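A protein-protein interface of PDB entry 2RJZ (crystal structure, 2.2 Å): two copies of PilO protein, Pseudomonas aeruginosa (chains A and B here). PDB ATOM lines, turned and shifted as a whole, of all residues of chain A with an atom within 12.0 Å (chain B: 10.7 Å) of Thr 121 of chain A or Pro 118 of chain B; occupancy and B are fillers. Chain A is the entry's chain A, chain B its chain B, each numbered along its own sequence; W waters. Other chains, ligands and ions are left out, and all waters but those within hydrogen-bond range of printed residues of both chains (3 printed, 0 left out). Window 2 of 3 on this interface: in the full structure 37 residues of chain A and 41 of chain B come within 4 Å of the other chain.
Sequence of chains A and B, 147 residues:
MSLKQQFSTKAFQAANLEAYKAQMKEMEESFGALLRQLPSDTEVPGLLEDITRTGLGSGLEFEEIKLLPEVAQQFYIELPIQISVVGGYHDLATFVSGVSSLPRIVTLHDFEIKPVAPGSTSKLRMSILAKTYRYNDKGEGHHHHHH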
ATOM      1  N   SER A  58       5.212 -25.176  15.122  1.00  0.00           N
ATOM      2  CA  SER A  58       4.221 -24.836  16.143  1.00  0.00           C
ATOM      3  C   SER A  58       4.155 -23.349  16.437  1.00  0.00           C
ATOM      4  O   SER A  58       3.394 -22.943  17.310  1.00  0.00           O
ATOM      5  CB  SER A  58       4.449 -25.613  17.439  1.00  0.00           C
ATOM      6  OG  SER A  58       4.487 -27.014  17.209  1.00  0.00           O
ATOM      7  N   GLY A  59       4.915 -22.532  15.710  1.00  0.00           N
ATOM      8  CA  GLY A  59       4.883 -21.077  15.929  1.00  0.00           C
ATOM      9  C   GLY A  59       5.703 -20.659  17.139  1.00  0.00           C
ATOM     10  O   GLY A  59       5.402 -19.677  17.816  1.00  0.00           O
ATOM     11  N   LEU A  60       6.747 -21.420  17.429  1.00  0.00           N
ATOM     12  CA  LEU A  60       7.601 -21.109  18.552  1.00  0.00           C
ATOM     13  C   LEU A  60       8.898 -20.507  18.030  1.00  0.00           C
ATOM     14  O   LEU A  60       9.330 -20.831  16.911  1.00  0.00           O
ATOM     15  CB  LEU A  60       7.913 -22.397  19.325  1.00  0.00           C
ATOM     16  CG  LEU A  60       6.770 -23.203  19.938  1.00  0.00           C
ATOM     17  CD1 LEU A  60       7.366 -24.341  20.706  1.00  0.00           C
ATOM     18  CD2 LEU A  60       5.923 -22.350  20.844  1.00  0.00           C
ATOM     19  N   VAL A  85      12.462 -22.588  24.490  1.00  0.00           N
ATOM     20  CA  VAL A  85      11.619 -22.024  23.448  1.00  0.00           C
ATOM     21  C   VAL A  85      10.694 -20.962  24.062  1.00  0.00           C
ATOM     22  O   VAL A  85      10.549 -20.889  25.284  1.00  0.00           O
ATOM     23  CB  VAL A  85      10.784 -23.119  22.737  1.00  0.00           C
ATOM     24  CG1 VAL A  85      11.692 -24.038  21.990  1.00  0.00           C
ATOM     25  CG2 VAL A  85       9.962 -23.927  23.733  1.00  0.00           C
ATOM     26  N   VAL A  86      10.097 -20.144  23.206  1.00  0.00           N
ATOM     27  CA  VAL A  86       9.193 -19.059  23.605  1.00  0.00           C
ATOM     28  C   VAL A  86       8.000 -19.121  22.630  1.00  0.00           C
ATOM     29  O   VAL A  86       8.197 -19.322  21.426  1.00  0.00           O
ATOM     30  CB  VAL A  86       9.893 -17.658  23.551  1.00  0.00           C
ATOM     31  CG1 VAL A  86       8.883 -16.505  23.753  1.00  0.00           C
ATOM     32  CG2 VAL A  86      10.981 -17.551  24.623  1.00  0.00           C
ATOM     33  N   GLY A  87       6.785 -19.036  23.170  1.00  0.00           N
ATOM     34  CA  GLY A  87       5.579 -18.873  22.368  1.00  0.00           C
ATOM     35  C   GLY A  87       4.316 -18.960  23.214  1.00  0.00           C
ATOM     36  O   GLY A  87       4.371 -18.834  24.441  1.00  0.00           O
ATOM     37  N   GLY A  88       3.176 -19.191  22.563  1.00  0.00           N
ATOM     38  CA  GLY A  88       1.874 -19.242  23.260  1.00  0.00           C
ATOM     39  C   GLY A  88       1.588 -20.578  23.920  1.00  0.00           C
ATOM     40  O   GLY A  88       2.209 -21.590  23.598  1.00  0.00           O
ATOM     41  N   TYR A  89       0.614 -20.591  24.824  1.00  0.00           N
ATOM     42  CA  TYR A  89       0.388 -21.769  25.658  1.00  0.00           C
ATOM     43  C   TYR A  89      -0.038 -23.050  24.913  1.00  0.00           C
ATOM     44  O   TYR A  89       0.415 -24.156  25.250  1.00  0.00           O
ATOM     45  CB  TYR A  89      -0.503 -21.433  26.872  1.00  0.00           C
ATOM     46  CG  TYR A  89      -1.894 -20.956  26.558  1.00  0.00           C
ATOM     47  CD1 TYR A  89      -2.915 -21.871  26.286  1.00  0.00           C
ATOM     48  CD2 TYR A  89      -2.208 -19.593  26.572  1.00  0.00           C
ATOM     49  CE1 TYR A  89      -4.234 -21.455  26.000  1.00  0.00           C
ATOM     50  CE2 TYR A  89      -3.544 -19.148  26.279  1.00  0.00           C
ATOM     51  CZ  TYR A  89      -4.537 -20.102  25.999  1.00  0.00           C
ATOM     52  OH  TYR A  89      -5.836 -19.726  25.727  1.00  0.00           O
ATOM     53  N   HIS A  90      -0.866 -22.893  23.883  1.00  0.00           N
ATOM     54  CA  HIS A  90      -1.305 -24.008  23.037  1.00  0.00           C
ATOM     55  C   HIS A  90      -0.124 -24.522  22.218  1.00  0.00           C
ATOM     56  O   HIS A  90       0.065 -25.731  22.072  1.00  0.00           O
ATOM     57  CB  HIS A  90      -2.450 -23.526  22.121  1.00  0.00           C
ATOM     58  CG  HIS A  90      -3.080 -24.607  21.293  1.00  0.00           C
ATOM     59  ND1 HIS A  90      -2.922 -24.688  19.919  1.00  0.00           N
ATOM     60  CD2 HIS A  90      -3.875 -25.647  21.642  1.00  0.00           C
ATOM     61  CE1 HIS A  90      -3.590 -25.734  19.461  1.00  0.00           C
ATOM     62  NE2 HIS A  90      -4.178 -26.332  20.486  1.00  0.00           N
ATOM     63  N   ASP A  91       0.688 -23.599  21.708  1.00  0.00           N
ATOM     64  CA  ASP A  91       1.778 -23.909  20.778  1.00  0.00           C
ATOM     65  C   ASP A  91       2.859 -24.748  21.483  1.00  0.00           C
ATOM     66  O   ASP A  91       3.352 -25.727  20.948  1.00  0.00           O
ATOM     67  CB  ASP A  91       2.357 -22.596  20.194  1.00  0.00           C
ATOM     68  CG  ASP A  91       1.434 -21.965  19.123  1.00  0.00           C
ATOM     69  OD1 ASP A  91       0.632 -22.716  18.497  1.00  0.00           O
ATOM     70  OD2 ASP A  91       1.517 -20.727  18.892  1.00  0.00           O
ATOM     71  N   LEU A  92       3.200 -24.347  22.703  1.00  0.00           N
ATOM     72  CA  LEU A  92       4.068 -25.145  23.582  1.00  0.00           C
ATOM     73  C   LEU A  92       3.641 -26.618  23.727  1.00  0.00           C
ATOM     74  O   LEU A  92       4.491 -27.524  23.687  1.00  0.00           O
ATOM     75  CB  LEU A  92       4.180 -24.493  24.976  1.00  0.00           C
ATOM     76  CG  LEU A  92       4.917 -23.156  25.025  1.00  0.00           C
ATOM     77  CD1 LEU A  92       4.768 -22.483  26.378  1.00  0.00           C
ATOM     78  CD2 LEU A  92       6.364 -23.308  24.636  1.00  0.00           C
ATOM     79  N   ALA A  93       2.341 -26.862  23.919  1.00  0.00           N
ATOM     80  CA  ALA A  93       1.873 -28.227  24.177  1.00  0.00           C
ATOM     81  C   ALA A  93       1.908 -29.041  22.892  1.00  0.00           C
ATOM     82  O   ALA A  93       2.275 -30.221  22.897  1.00  0.00           O
ATOM     83  CB  ALA A  93       0.449 -28.233  24.790  1.00  0.00           C
ATOM     84  N   ILE A 113       7.853 -23.685  32.835  1.00  0.00           N
ATOM     85  CA  ILE A 113       7.328 -22.582  32.053  1.00  0.00           C
ATOM     86  C   ILE A 113       7.361 -21.292  32.852  1.00  0.00           C
ATOM     87  O   ILE A 113       7.145 -21.294  34.059  1.00  0.00           O
ATOM     88  CB  ILE A 113       5.893 -22.919  31.573  1.00  0.00           C
ATOM     89  CG1 ILE A 113       5.954 -24.161  30.666  1.00  0.00           C
ATOM     90  CG2 ILE A 113       5.209 -21.721  30.905  1.00  0.00           C
ATOM     91  CD1 ILE A 113       4.631 -24.759  30.322  1.00  0.00           C
ATOM     92  N   LYS A 114       7.674 -20.197  32.166  1.00  0.00           N
ATOM     93  CA  LYS A 114       7.609 -18.862  32.745  1.00  0.00           C
ATOM     94  C   LYS A 114       7.163 -17.829  31.696  1.00  0.00           C
ATOM     95  O   LYS A 114       7.633 -17.866  30.570  1.00  0.00           O
ATOM     96  CB  LYS A 114       8.954 -18.467  33.348  1.00  0.00           C
ATOM     97  CG  LYS A 114       8.812 -17.479  34.512  1.00  0.00           C
ATOM     98  CD  LYS A 114      10.167 -17.034  35.103  1.00  0.00           C
ATOM     99  CE  LYS A 114       9.979 -15.759  35.972  1.00  0.00           C
ATOM    100  NZ  LYS A 114       9.047 -15.968  37.178  1.00  0.00           N
ATOM    101  N   PRO A 115       6.256 -16.906  32.067  1.00  0.00           N
ATOM    102  CA  PRO A 115       5.966 -15.735  31.218  1.00  0.00           C
ATOM    103  C   PRO A 115       7.209 -14.884  30.935  1.00  0.00           C
ATOM    104  O   PRO A 115       8.072 -14.713  31.808  1.00  0.00           O
ATOM    105  CB  PRO A 115       4.942 -14.929  32.039  1.00  0.00           C
ATOM    106  CG  PRO A 115       5.059 -15.462  33.446  1.00  0.00           C
ATOM    107  CD  PRO A 115       5.443 -16.905  33.291  1.00  0.00           C
ATOM    108  N   VAL A 116       7.287 -14.382  29.705  1.00  0.00           N
ATOM    109  CA  VAL A 116       8.383 -13.530  29.269  1.00  0.00           C
ATOM    110  C   VAL A 116       8.290 -12.138  29.883  1.00  0.00           C
ATOM    111  O   VAL A 116       9.299 -11.584  30.328  1.00  0.00           O
ATOM    112  CB  VAL A 116       8.462 -13.442  27.716  1.00  0.00           C
ATOM    113  CG1 VAL A 116       9.365 -12.292  27.278  1.00  0.00           C
ATOM    114  CG2 VAL A 116       8.989 -14.763  27.132  1.00  0.00           C
ATOM    115  N   ALA A 117       7.081 -11.591  29.925  1.00  0.00           N
ATOM    116  CA  ALA A 117       6.865 -10.221  30.366  1.00  0.00           C
ATOM    117  C   ALA A 117       5.678 -10.126  31.330  1.00  0.00           C
ATOM    118  O   ALA A 117       4.769 -10.963  31.267  1.00  0.00           O
ATOM    119  CB  ALA A 117       6.639  -9.333  29.157  1.00  0.00           C
ATOM    120  N   PRO A 118       5.667  -9.094  32.210  1.00  0.00           N
ATOM    121  CA  PRO A 118       4.519  -8.817  33.095  1.00  0.00           C
ATOM    122  C   PRO A 118       3.252  -8.533  32.293  1.00  0.00           C
ATOM    123  O   PRO A 118       3.308  -7.787  31.296  1.00  0.00           O
ATOM    124  CB  PRO A 118       4.941  -7.543  33.844  1.00  0.00           C
ATOM    125  CG  PRO A 118       6.004  -6.930  33.017  1.00  0.00           C
ATOM    126  CD  PRO A 118       6.738  -8.103  32.402  1.00  0.00           C
ATOM    127  N   GLY A 119       2.133  -9.123  32.715  1.00  0.00           N
ATOM    128  CA  GLY A 119       0.837  -8.942  32.046  1.00  0.00           C
ATOM    129  C   GLY A 119       0.609  -9.790  30.802  1.00  0.00           C
ATOM    130  O   GLY A 119      -0.484  -9.770  30.227  1.00  0.00           O
ATOM    131  N   SER A 120       1.641 -10.530  30.394  1.00  0.00           N
ATOM    132  CA  SER A 120       1.639 -11.310  29.147  1.00  0.00           C
ATOM    133  C   SER A 120       1.348 -12.763  29.433  1.00  0.00           C
ATOM    134  O   SER A 120       1.860 -13.330  30.411  1.00  0.00           O
ATOM    135  CB  SER A 120       3.001 -11.225  28.406  1.00  0.00           C
ATOM    136  OG  SER A 120       3.892 -12.300  28.752  1.00  0.00           O
ATOM    137  N   THR A 121       0.552 -13.357  28.546  1.00  0.00           N
ATOM    138  CA  THR A 121       0.240 -14.775  28.582  1.00  0.00           C
ATOM    139  C   THR A 121       0.325 -15.353  27.142  1.00  0.00           C
ATOM    140  O   THR A 121       0.169 -16.569  26.917  1.00  0.00           O
ATOM    141  CB  THR A 121      -1.135 -14.989  29.287  1.00  0.00           C
ATOM    142  OG1 THR A 121      -1.012 -15.979  30.325  1.00  0.00           O
ATOM    143  CG2 THR A 121      -2.270 -15.316  28.287  1.00  0.00           C
ATOM    144  N   SER A 122       0.604 -14.478  26.170  1.00  0.00           N
ATOM    145  CA  SER A 122       0.744 -14.904  24.763  1.00  0.00           C
ATOM    146  C   SER A 122       2.179 -15.286  24.430  1.00  0.00           C
ATOM    147  O   SER A 122       2.412 -16.022  23.465  1.00  0.00           O
ATOM    148  CB  SER A 122       0.223 -13.835  23.786  1.00  0.00           C
ATOM    149  OG  SER A 122       1.023 -12.666  23.833  1.00  0.00           O
ATOM    150  N   LYS A 123       3.139 -14.782  25.219  1.00  0.00           N
ATOM    151  CA  LYS A 123       4.509 -15.256  25.128  1.00  0.00           C
ATOM    152  C   LYS A 123       5.012 -15.878  26.447  1.00  0.00           C
ATOM    153  O   LYS A 123       5.295 -15.175  27.431  1.00  0.00           O
ATOM    154  CB  LYS A 123       5.454 -14.188  24.555  1.00  0.00           C
ATOM    155  CG  LYS A 123       5.477 -12.839  25.341  1.00  0.00           C
ATOM    156  CD  LYS A 123       6.203 -11.696  24.575  1.00  0.00           C
ATOM    157  CE  LYS A 123       5.197 -10.681  24.020  1.00  0.00           C
ATOM    158  NZ  LYS A 123       4.276 -10.217  25.123  1.00  0.00           N
ATOM    159  N   LEU A 124       5.111 -17.214  26.437  1.00  0.00           N
ATOM    160  CA  LEU A 124       5.715 -17.963  27.531  1.00  0.00           C
ATOM    161  C   LEU A 124       7.039 -18.626  27.137  1.00  0.00           C
ATOM    162  O   LEU A 124       7.228 -19.094  26.012  1.00  0.00           O
ATOM    163  CB  LEU A 124       4.746 -19.026  28.084  1.00  0.00           C
ATOM    164  CG  LEU A 124       3.288 -18.649  28.440  1.00  0.00           C
ATOM    165  CD1 LEU A 124       2.477 -19.912  28.772  1.00  0.00           C
ATOM    166  CD2 LEU A 124       3.191 -17.656  29.592  1.00  0.00           C
ATOM    167  N   ARG A 125       7.948 -18.671  28.101  1.00  0.00           N
ATOM    168  CA  ARG A 125       9.214 -19.334  27.935  1.00  0.00           C
ATOM    169  C   ARG A 125       9.111 -20.708  28.583  1.00  0.00           C
ATOM    170  O   ARG A 125       8.705 -20.803  29.744  1.00  0.00           O
ATOM    171  CB  ARG A 125      10.332 -18.505  28.583  1.00  0.00           C
ATOM    172  CG  ARG A 125      11.725 -19.052  28.335  1.00  0.00           C
ATOM    173  CD  ARG A 125      12.814 -18.041  28.767  1.00  0.00           C
ATOM    174  NE  ARG A 125      13.056 -17.027  27.739  1.00  0.00           N
ATOM    175  CZ  ARG A 125      12.881 -15.717  27.892  1.00  0.00           C
ATOM    176  NH1 ARG A 125      12.467 -15.215  29.054  1.00  0.00           N
ATOM    177  NH2 ARG A 125      13.137 -14.902  26.872  1.00  0.00           N
ATOM    178  N   MET A 126       9.453 -21.757  27.832  1.00  0.00           N
ATOM    179  CA  MET A 126       9.539 -23.115  28.366  1.00  0.00           C
ATOM    180  C   MET A 126      10.975 -23.633  28.232  1.00  0.00           C
ATOM    181  O   MET A 126      11.582 -23.551  27.151  1.00  0.00           O
ATOM    182  CB  MET A 126       8.601 -24.078  27.616  1.00  0.00           C
ATOM    183  CG  MET A 126       8.522 -25.513  28.251  1.00  0.00           C
ATOM    184  SD  MET A 126       7.345 -26.672  27.492  1.00  0.00           S
ATOM    185  CE  MET A 126       8.012 -26.763  25.846  1.00  0.00           C
ATOM    186  N   GLY B  87      -2.054 -23.784  39.865  1.00  0.00           N
ATOM    187  CA  GLY B  87      -1.078 -23.166  40.716  1.00  0.00           C
ATOM    188  C   GLY B  87      -0.158 -22.297  39.897  1.00  0.00           C
ATOM    189  O   GLY B  87      -0.385 -22.078  38.713  1.00  0.00           O
ATOM    190  N   TYR B  89       3.586 -20.989  38.230  1.00  0.00           N
ATOM    191  CA  TYR B  89       4.459 -21.533  37.193  1.00  0.00           C
ATOM    192  C   TYR B  89       5.548 -22.467  37.753  1.00  0.00           C
ATOM    193  O   TYR B  89       5.743 -23.572  37.253  1.00  0.00           O
ATOM    194  CB  TYR B  89       5.072 -20.368  36.397  1.00  0.00           C
ATOM    195  CG  TYR B  89       4.069 -19.724  35.447  1.00  0.00           C
ATOM    196  CD1 TYR B  89       3.848 -20.257  34.176  1.00  0.00           C
ATOM    197  CD2 TYR B  89       3.340 -18.593  35.814  1.00  0.00           C
ATOM    198  CE1 TYR B  89       2.929 -19.686  33.281  1.00  0.00           C
ATOM    199  CE2 TYR B  89       2.406 -18.005  34.923  1.00  0.00           C
ATOM    200  CZ  TYR B  89       2.213 -18.572  33.660  1.00  0.00           C
ATOM    201  OH  TYR B  89       1.307 -18.034  32.759  1.00  0.00           O
ATOM    202  N   ILE B 113      -2.115 -26.654  28.897  1.00  0.00           N
ATOM    203  CA  ILE B 113      -2.144 -25.563  29.873  1.00  0.00           C
ATOM    204  C   ILE B 113      -3.025 -24.394  29.418  1.00  0.00           C
ATOM    205  O   ILE B 113      -3.240 -24.183  28.225  1.00  0.00           O
ATOM    206  CB  ILE B 113      -0.729 -25.018  30.164  1.00  0.00           C
ATOM    207  CG1 ILE B 113       0.007 -24.772  28.820  1.00  0.00           C
ATOM    208  CG2 ILE B 113       0.008 -25.982  31.102  1.00  0.00           C
ATOM    209  CD1 ILE B 113       1.204 -23.838  28.879  1.00  0.00           C
ATOM    210  N   LYS B 114      -3.519 -23.636  30.381  1.00  0.00           N
ATOM    211  CA  LYS B 114      -4.317 -22.460  30.088  1.00  0.00           C
ATOM    212  C   LYS B 114      -4.294 -21.552  31.315  1.00  0.00           C
ATOM    213  O   LYS B 114      -4.373 -22.041  32.439  1.00  0.00           O
ATOM    214  CB  LYS B 114      -5.750 -22.861  29.741  1.00  0.00           C
ATOM    215  CG  LYS B 114      -6.564 -21.767  29.020  1.00  0.00           C
ATOM    216  CD  LYS B 114      -8.071 -22.060  29.090  1.00  0.00           C
ATOM    217  CE  LYS B 114      -8.857 -21.344  27.967  1.00  0.00           C
ATOM    218  NZ  LYS B 114     -10.348 -21.389  28.238  1.00  0.00           N
ATOM    219  N   PRO B 115      -4.168 -20.229  31.108  1.00  0.00           N
ATOM    220  CA  PRO B 115      -4.253 -19.296  32.233  1.00  0.00           C
ATOM    221  C   PRO B 115      -5.580 -19.415  32.947  1.00  0.00           C
ATOM    222  O   PRO B 115      -6.584 -19.803  32.343  1.00  0.00           O
ATOM    223  CB  PRO B 115      -4.154 -17.924  31.562  1.00  0.00           C
ATOM    224  CG  PRO B 115      -3.414 -18.195  30.313  1.00  0.00           C
ATOM    225  CD  PRO B 115      -3.924 -19.517  29.845  1.00  0.00           C
ATOM    226  N   VAL B 116      -5.551 -19.141  34.243  1.00  0.00           N
ATOM    227  CA  VAL B 116      -6.758 -18.939  35.036  1.00  0.00           C
ATOM    228  C   VAL B 116      -7.462 -17.658  34.536  1.00  0.00           C
ATOM    229  O   VAL B 116      -8.693 -17.628  34.404  1.00  0.00           O
ATOM    230  CB  VAL B 116      -6.410 -18.866  36.544  1.00  0.00           C
ATOM    231  CG1 VAL B 116      -7.365 -17.940  37.297  1.00  0.00           C
ATOM    232  CG2 VAL B 116      -6.434 -20.247  37.153  1.00  0.00           C
ATOM    233  N   ALA B 117      -6.657 -16.632  34.230  1.00  0.00           N
ATOM    234  CA  ALA B 117      -7.128 -15.329  33.733  1.00  0.00           C
ATOM    235  C   ALA B 117      -6.281 -14.903  32.532  1.00  0.00           C
ATOM    236  O   ALA B 117      -5.045 -14.826  32.642  1.00  0.00           O
ATOM    237  CB  ALA B 117      -7.045 -14.266  34.846  1.00  0.00           C
ATOM    238  N   PRO B 118      -6.940 -14.584  31.391  1.00  0.00           N
ATOM    239  CA  PRO B 118      -6.274 -14.445  30.066  1.00  0.00           C
ATOM    240  C   PRO B 118      -5.044 -13.530  30.048  1.00  0.00           C
ATOM    241  O   PRO B 118      -4.987 -12.549  30.796  1.00  0.00           O
ATOM    242  CB  PRO B 118      -7.376 -13.870  29.165  1.00  0.00           C
ATOM    243  CG  PRO B 118      -8.690 -14.269  29.839  1.00  0.00           C
ATOM    244  CD  PRO B 118      -8.394 -14.301  31.327  1.00  0.00           C
ATOM    245  N   THR B 121       0.496 -13.610  34.826  1.00  0.00           N
ATOM    246  CA  THR B 121       1.329 -14.428  35.706  1.00  0.00           C
ATOM    247  C   THR B 121       0.489 -15.139  36.780  1.00  0.00           C
ATOM    248  O   THR B 121      -0.747 -15.179  36.712  1.00  0.00           O
ATOM    249  CB  THR B 121       2.445 -13.605  36.428  1.00  0.00           C
ATOM    250  OG1 THR B 121       3.046 -12.673  35.529  1.00  0.00           O
ATOM    251  CG2 THR B 121       3.522 -14.546  36.952  1.00  0.00           C
ATOM    252  N   SER B 122       1.179 -15.654  37.793  1.00  0.00           N
ATOM    253  CA  SER B 122       0.577 -16.447  38.858  1.00  0.00           C
ATOM    254  C   SER B 122       0.015 -17.715  38.244  1.00  0.00           C
ATOM    255  O   SER B 122       0.778 -18.548  37.763  1.00  0.00           O
ATOM    256  CB  SER B 122      -0.485 -15.651  39.642  1.00  0.00           C
ATOM    257  OG  SER B 122      -0.058 -14.308  39.827  1.00  0.00           O
ATOM    258  N   LYS B 123      -1.308 -17.834  38.198  1.00  0.00           N
ATOM    259  CA  LYS B 123      -1.935 -19.121  37.949  1.00  0.00           C
ATOM    260  C   LYS B 123      -1.965 -19.590  36.489  1.00  0.00           C
ATOM    261  O   LYS B 123      -2.166 -18.815  35.551  1.00  0.00           O
ATOM    262  CB  LYS B 123      -3.332 -19.177  38.567  1.00  0.00           C
ATOM    263  CG  LYS B 123      -3.429 -18.667  39.988  1.00  0.00           C
ATOM    264  CD  LYS B 123      -2.517 -19.416  40.934  1.00  0.00           C
ATOM    265  CE  LYS B 123      -2.669 -18.899  42.369  1.00  0.00           C
ATOM    266  NZ  LYS B 123      -3.955 -19.364  42.998  1.00  0.00           N
ATOM    267  N   LEU B 124      -1.757 -20.889  36.346  1.00  0.00           N
ATOM    268  CA  LEU B 124      -1.915 -21.607  35.118  1.00  0.00           C
ATOM    269  C   LEU B 124      -2.698 -22.888  35.472  1.00  0.00           C
ATOM    270  O   LEU B 124      -2.521 -23.456  36.546  1.00  0.00           O
ATOM    271  CB  LEU B 124      -0.524 -21.906  34.549  1.00  0.00           C
ATOM    272  CG  LEU B 124      -0.365 -22.419  33.119  1.00  0.00           C
ATOM    273  CD1 LEU B 124      -0.792 -21.373  32.089  1.00  0.00           C
ATOM    274  CD2 LEU B 124       1.072 -22.898  32.883  1.00  0.00           C
ATOM    275  N   ARG B 125      -3.626 -23.298  34.624  1.00  0.00           N
ATOM    276  CA  ARG B 125      -4.245 -24.612  34.797  1.00  0.00           C
ATOM    277  C   ARG B 125      -3.490 -25.593  33.909  1.00  0.00           C
ATOM    278  O   ARG B 125      -3.206 -25.293  32.756  1.00  0.00           O
ATOM    279  CB  ARG B 125      -5.725 -24.611  34.438  1.00  0.00           C
ATOM    280  CG  ARG B 125      -6.501 -23.453  35.034  1.00  0.00           C
ATOM    281  CD  ARG B 125      -7.868 -23.297  34.385  1.00  0.00           C
ATOM    282  NE  ARG B 125      -8.727 -24.429  34.702  1.00  0.00           N
ATOM    283  CZ  ARG B 125      -9.463 -24.509  35.798  1.00  0.00           C
ATOM    284  NH1 ARG B 125      -9.466 -23.519  36.679  1.00  0.00           N
ATOM    285  NH2 ARG B 125     -10.210 -25.573  36.012  1.00  0.00           N
HETATM  286  O   HOH W   1      -2.722 -11.278  30.439  1.00  0.00           O
HETATM  287  O   HOH W   2       6.080 -24.673  34.923  1.00  0.00           O
HETATM  288  O   HOH W   3      -1.557 -25.909  26.058  1.00  0.00           O
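Water W2 bridges O of Tyr 89 of chain B (2.6 Å) and N of Ile 113 of chain A (2.9 Å).
Water W1 bridges the backbone carbonyl oxygen of Pro 118 of chain B (2.6 Å) and the backbone carbonyl oxygen of Gly 119 of chain A (2.7 Å).
Water W3 lies within hydrogen-bond range of O of Tyr 89 of chain A and N of Ile 113 of chain B.
Printed residues of chain B within 4 Å of Tyr 89 of chain A: Ile 113 (3.0 Å), Lys 114 (3.8 Å) and Pro 115 (3.6 Å).
Gly 119 of chain A touches none of the printed residues of chain B.
Ser 120 of chain A touches none of the printed residues of chain B.
Thr 121 of chain A touches just these residues of chain B: Tyr 89, Pro 115 and Pro 118.
Printed residues of chain A within 4 Å of Tyr 89 of chain B: Ile 113 (3.3 Å), Pro 115 (3.6 Å), Thr 121 (3.9 Å) and Leu 124 (3.7 Å).
No residue of chain A comes within 4 Å of Ala 117 of chain B.
Of chain A, only Thr 121 comes within 4 Å of Pro 118 of chain B.
Ile 113 of chain A touches its own counterpart, Ile 113 of chain B.
Thr 121 of chain A touches Tyr 89 of chain B, but with the chains exchanged Tyr 89 of chain A does not touch Thr 121 of chain B (10.5 Å).
Thr 121 of chain A touches Pro 118 of chain B, but with the chains exchanged Pro 118 of chain A does not touch Thr 121 of chain B (4.8 Å).
Leu 124 of chain A touches Tyr 89 of chain B, but with the chains exchanged Tyr 89 of chain A does not touch Leu 124 of chain B (5.2 Å).
13 positions are printed for both chains.
Of the 11 pairs that touch across the chains among the printed residues, 7 have their exchanged pair printed and touching as well.
N of Leu 124 of chain A is in hydrogen-bond range of O of Gly 87 of chain A.
The backbone NH (N) of Arg 125 of chain B is in hydrogen-bond range of the backbone carbonyl oxygen (O) of Lys 114 of chain B.
CD1 of Tyr 89 of chain A touches O of Ile 113 of chain B, 3.0 Å away.
Tyr 89 of chain A touches Lys 114 of chain B (CE1 to CG, 3.8 Å).
CE2 of Tyr 89 of chain A touches CD of Pro 115 of chain B, 3.6 Å away.
O of Ile 113 of chain A touches CB of Tyr 89 of chain B, 3.3 Å away.
Ile 113 of chain B touches Ile 113 of chain A.
Tyr 89 of chain B touches Pro 115 of chain A.
Thr 121 of chain B touches Pro 115 of chain A (CG2 to CG, 3.9 Å).
Pro 115 of chain B touches Thr 121 of chain A.
CG2 of Thr 121 of chain A touches C of Pro 118 of chain B, at 3.7 Å.
CD2 of Leu 124 of chain A touches OH of Tyr 89 of chain B, 3.7 Å away.
Of the 26 printed residues of chain A, 5 touch a printed residue of chain B.
Hydrophobic or aromatic side chains of chain A that line the printed part of chain B: Tyr 89, Ile 113, Pro 115 and Leu 124.
Along chain A the printed residues that touch a printed residue of chain B span positions 89 to 124.
Of the 13 printed residues of chain B, 6 touch a printed residue of chain A.
Hydrophobic or aromatic side chains of chain B that line the printed part of chain A: Tyr 89, Ile 113 and Pro 115.
Among the printed residues, 11 pairs touch across the chains.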
